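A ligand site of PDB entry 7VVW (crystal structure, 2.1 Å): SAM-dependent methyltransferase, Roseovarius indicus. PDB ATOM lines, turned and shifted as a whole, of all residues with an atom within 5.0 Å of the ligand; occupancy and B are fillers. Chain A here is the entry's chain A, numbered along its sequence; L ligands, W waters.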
ATOM      1  N   ASP A  22      -5.205  15.786  -4.866  1.00  0.00           N
ATOM      2  CA  ASP A  22      -5.555  16.122  -3.530  1.00  0.00           C
ATOM      3  C   ASP A  22      -4.572  15.558  -2.550  1.00  0.00           C
ATOM      4  O   ASP A  22      -4.507  14.446  -2.329  1.00  0.00           O
ATOM      5  CB  ASP A  22      -6.908  15.570  -3.293  1.00  0.00           C
ATOM      6  CG  ASP A  22      -7.383  15.794  -1.926  1.00  0.00           C
ATOM      7  OD1 ASP A  22      -6.741  16.350  -1.121  1.00  0.00           O
ATOM      8  OD2 ASP A  22      -8.423  15.363  -1.631  1.00  0.00           O
ATOM      9  N   TRP A  24      -4.513  15.471   0.658  1.00  0.00           N
ATOM     10  CA  TRP A  24      -5.103  14.749   1.785  1.00  0.00           C
ATOM     11  C   TRP A  24      -5.410  13.304   1.404  1.00  0.00           C
ATOM     12  O   TRP A  24      -5.088  12.375   2.162  1.00  0.00           O
ATOM     13  CB  TRP A  24      -6.386  15.449   2.247  1.00  0.00           C
ATOM     14  CG  TRP A  24      -6.201  16.694   3.061  1.00  0.00           C
ATOM     15  CD1 TRP A  24      -5.633  17.862   2.658  1.00  0.00           C
ATOM     16  CD2 TRP A  24      -6.565  16.876   4.439  1.00  0.00           C
ATOM     17  NE1 TRP A  24      -5.635  18.771   3.698  1.00  0.00           N
ATOM     18  CE2 TRP A  24      -6.219  18.200   4.793  1.00  0.00           C
ATOM     19  CE3 TRP A  24      -7.173  16.062   5.400  1.00  0.00           C
ATOM     20  CZ2 TRP A  24      -6.446  18.727   6.065  1.00  0.00           C
ATOM     21  CZ3 TRP A  24      -7.424  16.596   6.670  1.00  0.00           C
ATOM     22  CH2 TRP A  24      -7.056  17.910   6.990  1.00  0.00           C
ATOM     23  N   VAL A  45     -15.609   3.952   6.373  1.00  0.00           N
ATOM     24  CA  VAL A  45     -16.642   4.901   6.758  1.00  0.00           C
ATOM     25  C   VAL A  45     -16.534   6.125   5.843  1.00  0.00           C
ATOM     26  O   VAL A  45     -15.507   6.798   5.813  1.00  0.00           O
ATOM     27  CB  VAL A  45     -16.514   5.310   8.237  1.00  0.00           C
ATOM     28  CG1 VAL A  45     -17.649   6.214   8.615  1.00  0.00           C
ATOM     29  CG2 VAL A  45     -16.501   4.096   9.127  1.00  0.00           C
ATOM     30  N   GLY A  46     -17.600   6.381   5.081  1.00  0.00           N
ATOM     31  CA  GLY A  46     -17.654   7.506   4.161  1.00  0.00           C
ATOM     32  C   GLY A  46     -17.071   7.211   2.782  1.00  0.00           C
ATOM     33  O   GLY A  46     -16.196   7.947   2.310  1.00  0.00           O
ATOM     34  N   ILE A  47     -17.569   6.159   2.116  1.00  0.00           N
ATOM     35  CA  ILE A  47     -17.000   5.717   0.837  1.00  0.00           C
ATOM     36  C   ILE A  47     -17.067   6.787  -0.241  1.00  0.00           C
ATOM     37  O   ILE A  47     -16.238   6.792  -1.164  1.00  0.00           O
ATOM     38  CB  ILE A  47     -17.701   4.441   0.339  1.00  0.00           C
ATOM     39  CG1 ILE A  47     -19.216   4.605   0.456  1.00  0.00           C
ATOM     40  CG2 ILE A  47     -17.205   3.227   1.121  1.00  0.00           C
ATOM     41  CD1 ILE A  47     -20.003   3.476  -0.185  1.00  0.00           C
ATOM     42  N   GLY A  48     -18.055   7.685  -0.186  1.00  0.00           N
ATOM     43  CA  GLY A  48     -18.149   8.704  -1.224  1.00  0.00           C
ATOM     44  C   GLY A  48     -18.425   8.058  -2.577  1.00  0.00           C
ATOM     45  O   GLY A  48     -19.290   7.177  -2.691  1.00  0.00           O
ATOM     46  N   ASP A  69     -21.953   5.374   3.626  1.00  0.00           N
ATOM     47  CA  ASP A  69     -21.840   6.816   3.594  1.00  0.00           C
ATOM     48  C   ASP A  69     -23.124   7.421   4.132  1.00  0.00           C
ATOM     49  O   ASP A  69     -24.192   6.803   4.115  1.00  0.00           O
ATOM     50  CB  ASP A  69     -21.552   7.315   2.178  1.00  0.00           C
ATOM     51  CG  ASP A  69     -21.029   8.732   2.156  1.00  0.00           C
ATOM     52  OD1 ASP A  69     -21.852   9.674   2.393  1.00  0.00           O
ATOM     53  OD2 ASP A  69     -19.823   8.912   1.887  1.00  0.00           O
ATOM     54  N   LEU A  70     -23.044   8.633   4.577  1.00  0.00           N
ATOM     55  CA  LEU A  70     -24.169   9.334   5.083  1.00  0.00           C
ATOM     56  C   LEU A  70     -25.204   9.556   4.023  1.00  0.00           C
ATOM     57  O   LEU A  70     -26.320   9.369   4.250  1.00  0.00           O
ATOM     58  CB  LEU A  70     -23.699  10.646   5.620  1.00  0.00           C
ATOM     59  CG  LEU A  70     -24.660  11.539   6.299  1.00  0.00           C
ATOM     60  CD1 LEU A  70     -25.241  10.860   7.491  1.00  0.00           C
ATOM     61  CD2 LEU A  70     -23.883  12.712   6.741  1.00  0.00           C
ATOM     62  N   ASP A  71     -24.803   9.940   2.854  1.00  0.00           N
ATOM     63  CA  ASP A  71     -25.699  10.120   1.718  1.00  0.00           C
ATOM     64  C   ASP A  71     -26.073   8.777   1.094  1.00  0.00           C
ATOM     65  O   ASP A  71     -25.186   8.072   0.597  1.00  0.00           O
ATOM     66  CB  ASP A  71     -25.024  11.013   0.694  1.00  0.00           C
ATOM     67  CG  ASP A  71     -25.943  11.488  -0.405  1.00  0.00           C
ATOM     68  OD1 ASP A  71     -26.778  10.705  -0.914  1.00  0.00           O
ATOM     69  OD2 ASP A  71     -25.792  12.665  -0.788  1.00  0.00           O
ATOM     70  N   LEU A  74     -24.730   7.479  -2.663  1.00  0.00           N
ATOM     71  CA  LEU A  74     -23.352   7.153  -2.958  1.00  0.00           C
ATOM     72  C   LEU A  74     -23.001   5.705  -3.087  1.00  0.00           C
ATOM     73  O   LEU A  74     -22.184   5.356  -3.846  1.00  0.00           O
ATOM     74  CB  LEU A  74     -22.452   7.854  -2.010  1.00  0.00           C
ATOM     75  CG  LEU A  74     -22.636   9.320  -2.026  1.00  0.00           C
ATOM     76  CD1 LEU A  74     -21.813   9.894  -0.956  1.00  0.00           C
ATOM     77  CD2 LEU A  74     -22.169   9.899  -3.298  1.00  0.00           C
ATOM     78  N   VAL A 100     -26.152   5.956   6.201  1.00  0.00           N
ATOM     79  CA  VAL A 100     -25.465   5.443   7.379  1.00  0.00           C
ATOM     80  C   VAL A 100     -24.555   6.537   7.897  1.00  0.00           C
ATOM     81  O   VAL A 100     -23.557   6.881   7.253  1.00  0.00           O
ATOM     82  CB  VAL A 100     -24.666   4.172   7.055  1.00  0.00           C
ATOM     83  CG1 VAL A 100     -23.928   3.705   8.303  1.00  0.00           C
ATOM     84  CG2 VAL A 100     -25.585   3.100   6.460  1.00  0.00           C
ATOM     85  N   SER A 101     -24.874   7.089   9.067  1.00  0.00           N
ATOM     86  CA  SER A 101     -23.984   8.011   9.743  1.00  0.00           C
ATOM     87  C   SER A 101     -23.010   7.206  10.607  1.00  0.00           C
ATOM     88  O   SER A 101     -23.438   6.384  11.419  1.00  0.00           O
ATOM     89  CB  SER A 101     -24.760   9.012  10.602  1.00  0.00           C
ATOM     90  OG  SER A 101     -23.844   9.823  11.326  1.00  0.00           O
ATOM     91  N   LEU A 102     -21.712   7.436  10.400  1.00  0.00           N
ATOM     92  CA  LEU A 102     -20.648   6.627  10.976  1.00  0.00           C
ATOM     93  C   LEU A 102     -20.973   5.176  10.627  1.00  0.00           C
ATOM     94  O   LEU A 102     -20.953   4.805   9.436  1.00  0.00           O
ATOM     95  CB  LEU A 102     -20.543   6.873  12.498  1.00  0.00           C
ATOM     96  CG  LEU A 102     -20.127   8.321  12.826  1.00  0.00           C
ATOM     97  CD1 LEU A 102     -19.869   8.602  14.322  1.00  0.00           C
ATOM     98  CD2 LEU A 102     -18.912   8.710  11.983  1.00  0.00           C
ATOM     99  N   CYS A 121     -11.469   8.819   6.148  1.00  0.00           N
ATOM    100  CA  CYS A 121     -10.911  10.162   6.108  1.00  0.00           C
ATOM    101  C   CYS A 121     -12.104  11.083   6.354  1.00  0.00           C
ATOM    102  O   CYS A 121     -12.876  11.349   5.433  1.00  0.00           O
ATOM    103  CB  CYS A 121     -10.198  10.448   4.786  1.00  0.00           C
ATOM    104  SG  CYS A 121      -9.481  12.105   4.729  1.00  0.00           S
ATOM    105  N   LEU A 122     -12.249  11.535   7.605  1.00  0.00           N
ATOM    106  CA  LEU A 122     -13.530  12.000   8.123  1.00  0.00           C
ATOM    107  C   LEU A 122     -13.528  13.507   8.386  1.00  0.00           C
ATOM    108  O   LEU A 122     -12.471  14.100   8.607  1.00  0.00           O
ATOM    109  CB  LEU A 122     -13.870  11.274   9.434  1.00  0.00           C
ATOM    110  CG  LEU A 122     -14.719   9.988   9.316  1.00  0.00           C
ATOM    111  CD1 LEU A 122     -14.319   9.176   8.141  1.00  0.00           C
ATOM    112  CD2 LEU A 122     -14.592   9.148  10.563  1.00  0.00           C
ATOM    113  N   PRO A 123     -14.711  14.133   8.359  1.00  0.00           N
ATOM    114  CA  PRO A 123     -14.798  15.576   8.653  1.00  0.00           C
ATOM    115  C   PRO A 123     -14.080  15.943   9.949  1.00  0.00           C
ATOM    116  O   PRO A 123     -14.106  15.210  10.937  1.00  0.00           O
ATOM    117  CB  PRO A 123     -16.308  15.813   8.757  1.00  0.00           C
ATOM    118  CG  PRO A 123     -16.911  14.792   7.870  1.00  0.00           C
ATOM    119  CD  PRO A 123     -16.014  13.580   7.947  1.00  0.00           C
ATOM    120  N   GLN A 124     -13.426  17.093   9.910  1.00  0.00           N
ATOM    121  CA  GLN A 124     -12.663  17.546  11.068  1.00  0.00           C
ATOM    122  C   GLN A 124     -12.380  19.026  10.870  1.00  0.00           C
ATOM    123  O   GLN A 124     -12.291  19.506   9.743  1.00  0.00           O
ATOM    124  CB  GLN A 124     -11.353  16.747  11.221  1.00  0.00           C
ATOM    125  CG  GLN A 124     -10.448  16.782   9.985  1.00  0.00           C
ATOM    126  CD  GLN A 124      -9.363  15.703  10.011  1.00  0.00           C
ATOM    127  OE1 GLN A 124      -8.200  15.978  10.342  1.00  0.00           O
ATOM    128  NE2 GLN A 124      -9.741  14.477   9.675  1.00  0.00           N
ATOM    129  N   GLU A 127      -9.928  20.559   8.061  1.00  0.00           N
ATOM    130  CA  GLU A 127     -10.130  20.036   6.710  1.00  0.00           C
ATOM    131  C   GLU A 127     -10.126  21.187   5.692  1.00  0.00           C
ATOM    132  O   GLU A 127     -10.384  22.334   6.050  1.00  0.00           O
ATOM    133  CB  GLU A 127     -11.471  19.287   6.633  1.00  0.00           C
ATOM    134  CG  GLU A 127     -12.661  20.260   6.547  1.00  0.00           C
ATOM    135  CD  GLU A 127     -13.987  19.645   6.965  1.00  0.00           C
ATOM    136  OE1 GLU A 127     -13.998  18.471   7.382  1.00  0.00           O
ATOM    137  OE2 GLU A 127     -15.016  20.339   6.869  1.00  0.00           O
ATOM    138  N   PRO A 128      -9.822  20.901   4.419  1.00  0.00           N
ATOM    139  CA  PRO A 128      -9.814  21.970   3.411  1.00  0.00           C
ATOM    140  C   PRO A 128     -11.164  22.674   3.365  1.00  0.00           C
ATOM    141  O   PRO A 128     -12.221  22.037   3.461  1.00  0.00           O
ATOM    142  CB  PRO A 128      -9.516  21.224   2.094  1.00  0.00           C
ATOM    143  CG  PRO A 128      -8.836  19.974   2.500  1.00  0.00           C
ATOM    144  CD  PRO A 128      -9.438  19.592   3.838  1.00  0.00           C
ATOM    145  N   VAL A 131     -14.029  21.381   1.056  1.00  0.00           N
ATOM    146  CA  VAL A 131     -14.256  19.949   0.947  1.00  0.00           C
ATOM    147  C   VAL A 131     -15.747  19.626   0.926  1.00  0.00           C
ATOM    148  O   VAL A 131     -16.174  18.663   0.291  1.00  0.00           O
ATOM    149  CB  VAL A 131     -13.527  19.205   2.086  1.00  0.00           C
ATOM    150  CG1 VAL A 131     -14.326  19.275   3.396  1.00  0.00           C
ATOM    151  CG2 VAL A 131     -13.235  17.791   1.681  1.00  0.00           C
ATOM    152  N   ALA A 135     -17.482  17.802  -2.138  1.00  0.00           N
ATOM    153  CA  ALA A 135     -18.205  16.556  -1.906  1.00  0.00           C
ATOM    154  C   ALA A 135     -19.625  16.631  -2.480  1.00  0.00           C
ATOM    155  O   ALA A 135     -20.125  15.652  -3.041  1.00  0.00           O
ATOM    156  CB  ALA A 135     -18.267  16.247  -0.410  1.00  0.00           C
ATOM    157  N   TRP A 162     -23.814  17.147   8.005  1.00  0.00           N
ATOM    158  CA  TRP A 162     -22.597  16.837   8.681  1.00  0.00           C
ATOM    159  C   TRP A 162     -22.776  17.295  10.121  1.00  0.00           C
ATOM    160  O   TRP A 162     -22.650  18.445  10.438  1.00  0.00           O
ATOM    161  CB  TRP A 162     -21.399  17.498   8.011  1.00  0.00           C
ATOM    162  CG  TRP A 162     -21.011  16.910   6.744  1.00  0.00           C
ATOM    163  CD1 TRP A 162     -21.761  16.210   5.959  1.00  0.00           C
ATOM    164  CD2 TRP A 162     -19.753  16.992   6.149  1.00  0.00           C
ATOM    165  NE1 TRP A 162     -21.080  15.823   4.881  1.00  0.00           N
ATOM    166  CE2 TRP A 162     -19.832  16.320   4.969  1.00  0.00           C
ATOM    167  CE3 TRP A 162     -18.582  17.611   6.491  1.00  0.00           C
ATOM    168  CZ2 TRP A 162     -18.793  16.220   4.134  1.00  0.00           C
ATOM    169  CZ3 TRP A 162     -17.570  17.510   5.669  1.00  0.00           C
ATOM    170  CH2 TRP A 162     -17.659  16.811   4.512  1.00  0.00           C
ATOM    171  N   PHE A 165     -21.305  16.547  16.820  1.00  0.00           N
ATOM    172  CA  PHE A 165     -20.598  15.696  17.763  1.00  0.00           C
ATOM    173  C   PHE A 165     -19.850  16.613  18.710  1.00  0.00           C
ATOM    174  O   PHE A 165     -18.666  16.425  18.962  1.00  0.00           O
ATOM    175  CB  PHE A 165     -19.622  14.769  17.036  1.00  0.00           C
ATOM    176  CG  PHE A 165     -20.296  13.789  16.107  1.00  0.00           C
ATOM    177  CD1 PHE A 165     -20.751  12.574  16.586  1.00  0.00           C
ATOM    178  CD2 PHE A 165     -20.473  14.093  14.766  1.00  0.00           C
ATOM    179  CE1 PHE A 165     -21.367  11.677  15.734  1.00  0.00           C
ATOM    180  CE2 PHE A 165     -21.089  13.196  13.914  1.00  0.00           C
ATOM    181  CZ  PHE A 165     -21.531  11.984  14.397  1.00  0.00           C
ATOM    182  N   LEU A 177     -16.005  14.136  15.711  1.00  0.00           N
ATOM    183  CA  LEU A 177     -16.511  13.062  14.858  1.00  0.00           C
ATOM    184  C   LEU A 177     -15.590  11.834  14.894  1.00  0.00           C
ATOM    185  O   LEU A 177     -16.062  10.690  14.972  1.00  0.00           O
ATOM    186  CB  LEU A 177     -16.686  13.563  13.422  1.00  0.00           C
ATOM    187  CG  LEU A 177     -17.620  12.718  12.563  1.00  0.00           C
ATOM    188  CD1 LEU A 177     -18.152  13.541  11.405  1.00  0.00           C
ATOM    189  CD2 LEU A 177     -16.864  11.590  11.971  1.00  0.00           C
HETATM  190  N1  LIG L   1     -11.147  16.087   5.340  1.00  0.00           N
HETATM  191  C1  LIG L   1     -11.909  15.009   4.732  1.00  0.00           C
HETATM  192  C2  LIG L   1     -11.162  14.496   3.483  1.00  0.00           C
HETATM  193  O1  LIG L   1     -11.243  13.303   3.234  1.00  0.00           O
HETATM  194  O2  LIG L   1     -10.480  15.208   2.719  1.00  0.00           O
HETATM  195  C3  LIG L   1     -13.319  15.472   4.365  1.00  0.00           C
HETATM  196  C4  LIG L   1     -14.477  14.460   4.499  1.00  0.00           C
HETATM  197  S1  LIG L   1     -15.054  13.725   2.941  1.00  0.00           S
HETATM  198  C5  LIG L   1     -15.385  15.116   1.817  1.00  0.00           C
HETATM  199  C6  LIG L   1     -16.794  13.416   3.317  1.00  0.00           C
HETATM  200  C7  LIG L   1     -17.285  12.065   2.841  1.00  0.00           C
HETATM  201  O3  LIG L   1     -17.615  11.364   4.020  1.00  0.00           O
HETATM  202  C8  LIG L   1     -18.573  12.274   2.069  1.00  0.00           C
HETATM  203  O4  LIG L   1     -18.762  11.194   1.174  1.00  0.00           O
HETATM  204  C9  LIG L   1     -19.612  12.269   3.169  1.00  0.00           C
HETATM  205  O5  LIG L   1     -20.891  11.853   2.742  1.00  0.00           O
HETATM  206  C10 LIG L   1     -19.011  11.278   4.167  1.00  0.00           C
HETATM  207  N2  LIG L   1     -19.417  11.617   5.538  1.00  0.00           N
HETATM  208  C11 LIG L   1     -19.441  12.849   6.123  1.00  0.00           C
HETATM  209  N3  LIG L   1     -19.891  12.700   7.399  1.00  0.00           N
HETATM  210  C12 LIG L   1     -20.156  11.394   7.607  1.00  0.00           C
HETATM  211  C13 LIG L   1     -20.635  10.687   8.688  1.00  0.00           C
HETATM  212  N4  LIG L   1     -20.934  11.323   9.821  1.00  0.00           N
HETATM  213  N5  LIG L   1     -20.796   9.321   8.596  1.00  0.00           N
HETATM  214  C14 LIG L   1     -20.496   8.653   7.433  1.00  0.00           C
HETATM  215  N6  LIG L   1     -20.021   9.364   6.360  1.00  0.00           N
HETATM  216  C15 LIG L   1     -19.859  10.701   6.444  1.00  0.00           C
HETATM  217  O   HOH W   1     -21.035   5.606   6.852  1.00  0.00           O
HETATM  218  O   HOH W   2     -20.784  14.124   9.574  1.00  0.00           O
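CE3 of Trp 24 touches N1 of the ligand, at 3.97 Å.
CG1 of Val 45 touches C14 of the ligand, at 3.9 Å.
Gly 46 touches the ligand (CA to N6, 3.7 Å).
Gly 48 touches the ligand (CA to O4, 3.5 Å).
Leu 70 touches the ligand.
CD1 of Leu 74 touches O4 of the ligand, at 3.9 Å.
Val 100 touches the ligand.
Ser 101 touches the ligand.
Pro 123 touches the ligand.
CB of Glu 127 touches N1 of the ligand, at 3.5 Å.
CG2 of Val 131 touches C5 of the ligand, 3.4 Å away.
Ala 135 touches the ligand.
Trp 162 touches the ligand (CZ2 to C6, 3.5 Å).
CD1 of Leu 177 touches N4 of the ligand (3.9 Å).
Hydrophobic or aromatic side chains that line the ligand: Trp 24, Val 45, Leu 70, Leu 74, Leu 102, Pro 123, Val 131, Ala 135, Trp 162 and Leu 177.
Within 4 Å of the ligand: Trp 24, Val 45, Gly 46, Gly 48, Asp 69, Leu 70, Leu 74, Val 100, Ser 101, Leu 102, Cys 121, Pro 123, Glu 127, Val 131, Ala 135, Trp 162 and Leu 177.
The nearest printed residue that does not touch the ligand is Leu 122 (4.02 Å).
N of Trp 24 sits at hydrogen-bond distance from OD1 of Asp 22 (3.0 Å).
OD2 of Asp 69 is in hydrogen-bond range of N of Gly 48 (3.0 Å).
OD1 of Asp 69 is in hydrogen-bond range of N of Asp 71 (3.0 Å).
The backbone carbonyl oxygen of Val 100 sits at hydrogen-bond distance from the backbone NH of Leu 70, at 3.2 Å.
The backbone NH (N) of Val 100 sits at hydrogen-bond distance from the backbone carbonyl oxygen (O) of Asp 69, at 3.0 Å.
The backbone NH (N) of Gln 124 sits at hydrogen-bond distance from the side-chain carboxylate (OE1) of Glu 127, at 2.9 Å.
The side-chain sulfur (SG) of Cys 121 is in hydrogen-bond range of an oxygen (O1) of the ligand (2.6 Å).
N of Leu 102 sits at hydrogen-bond distance from N5 of the ligand (2.8 Å).
The side-chain carboxylate (OD1) of Asp 69 sits at hydrogen-bond distance from an oxygen (O5) of the ligand, 2.4 Å away.
Water W1 lies within hydrogen-bond range of O of Leu 102 (2.7 Å), O of Val 100 (2.9 Å) and N of Asp 69 (3.4 Å).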
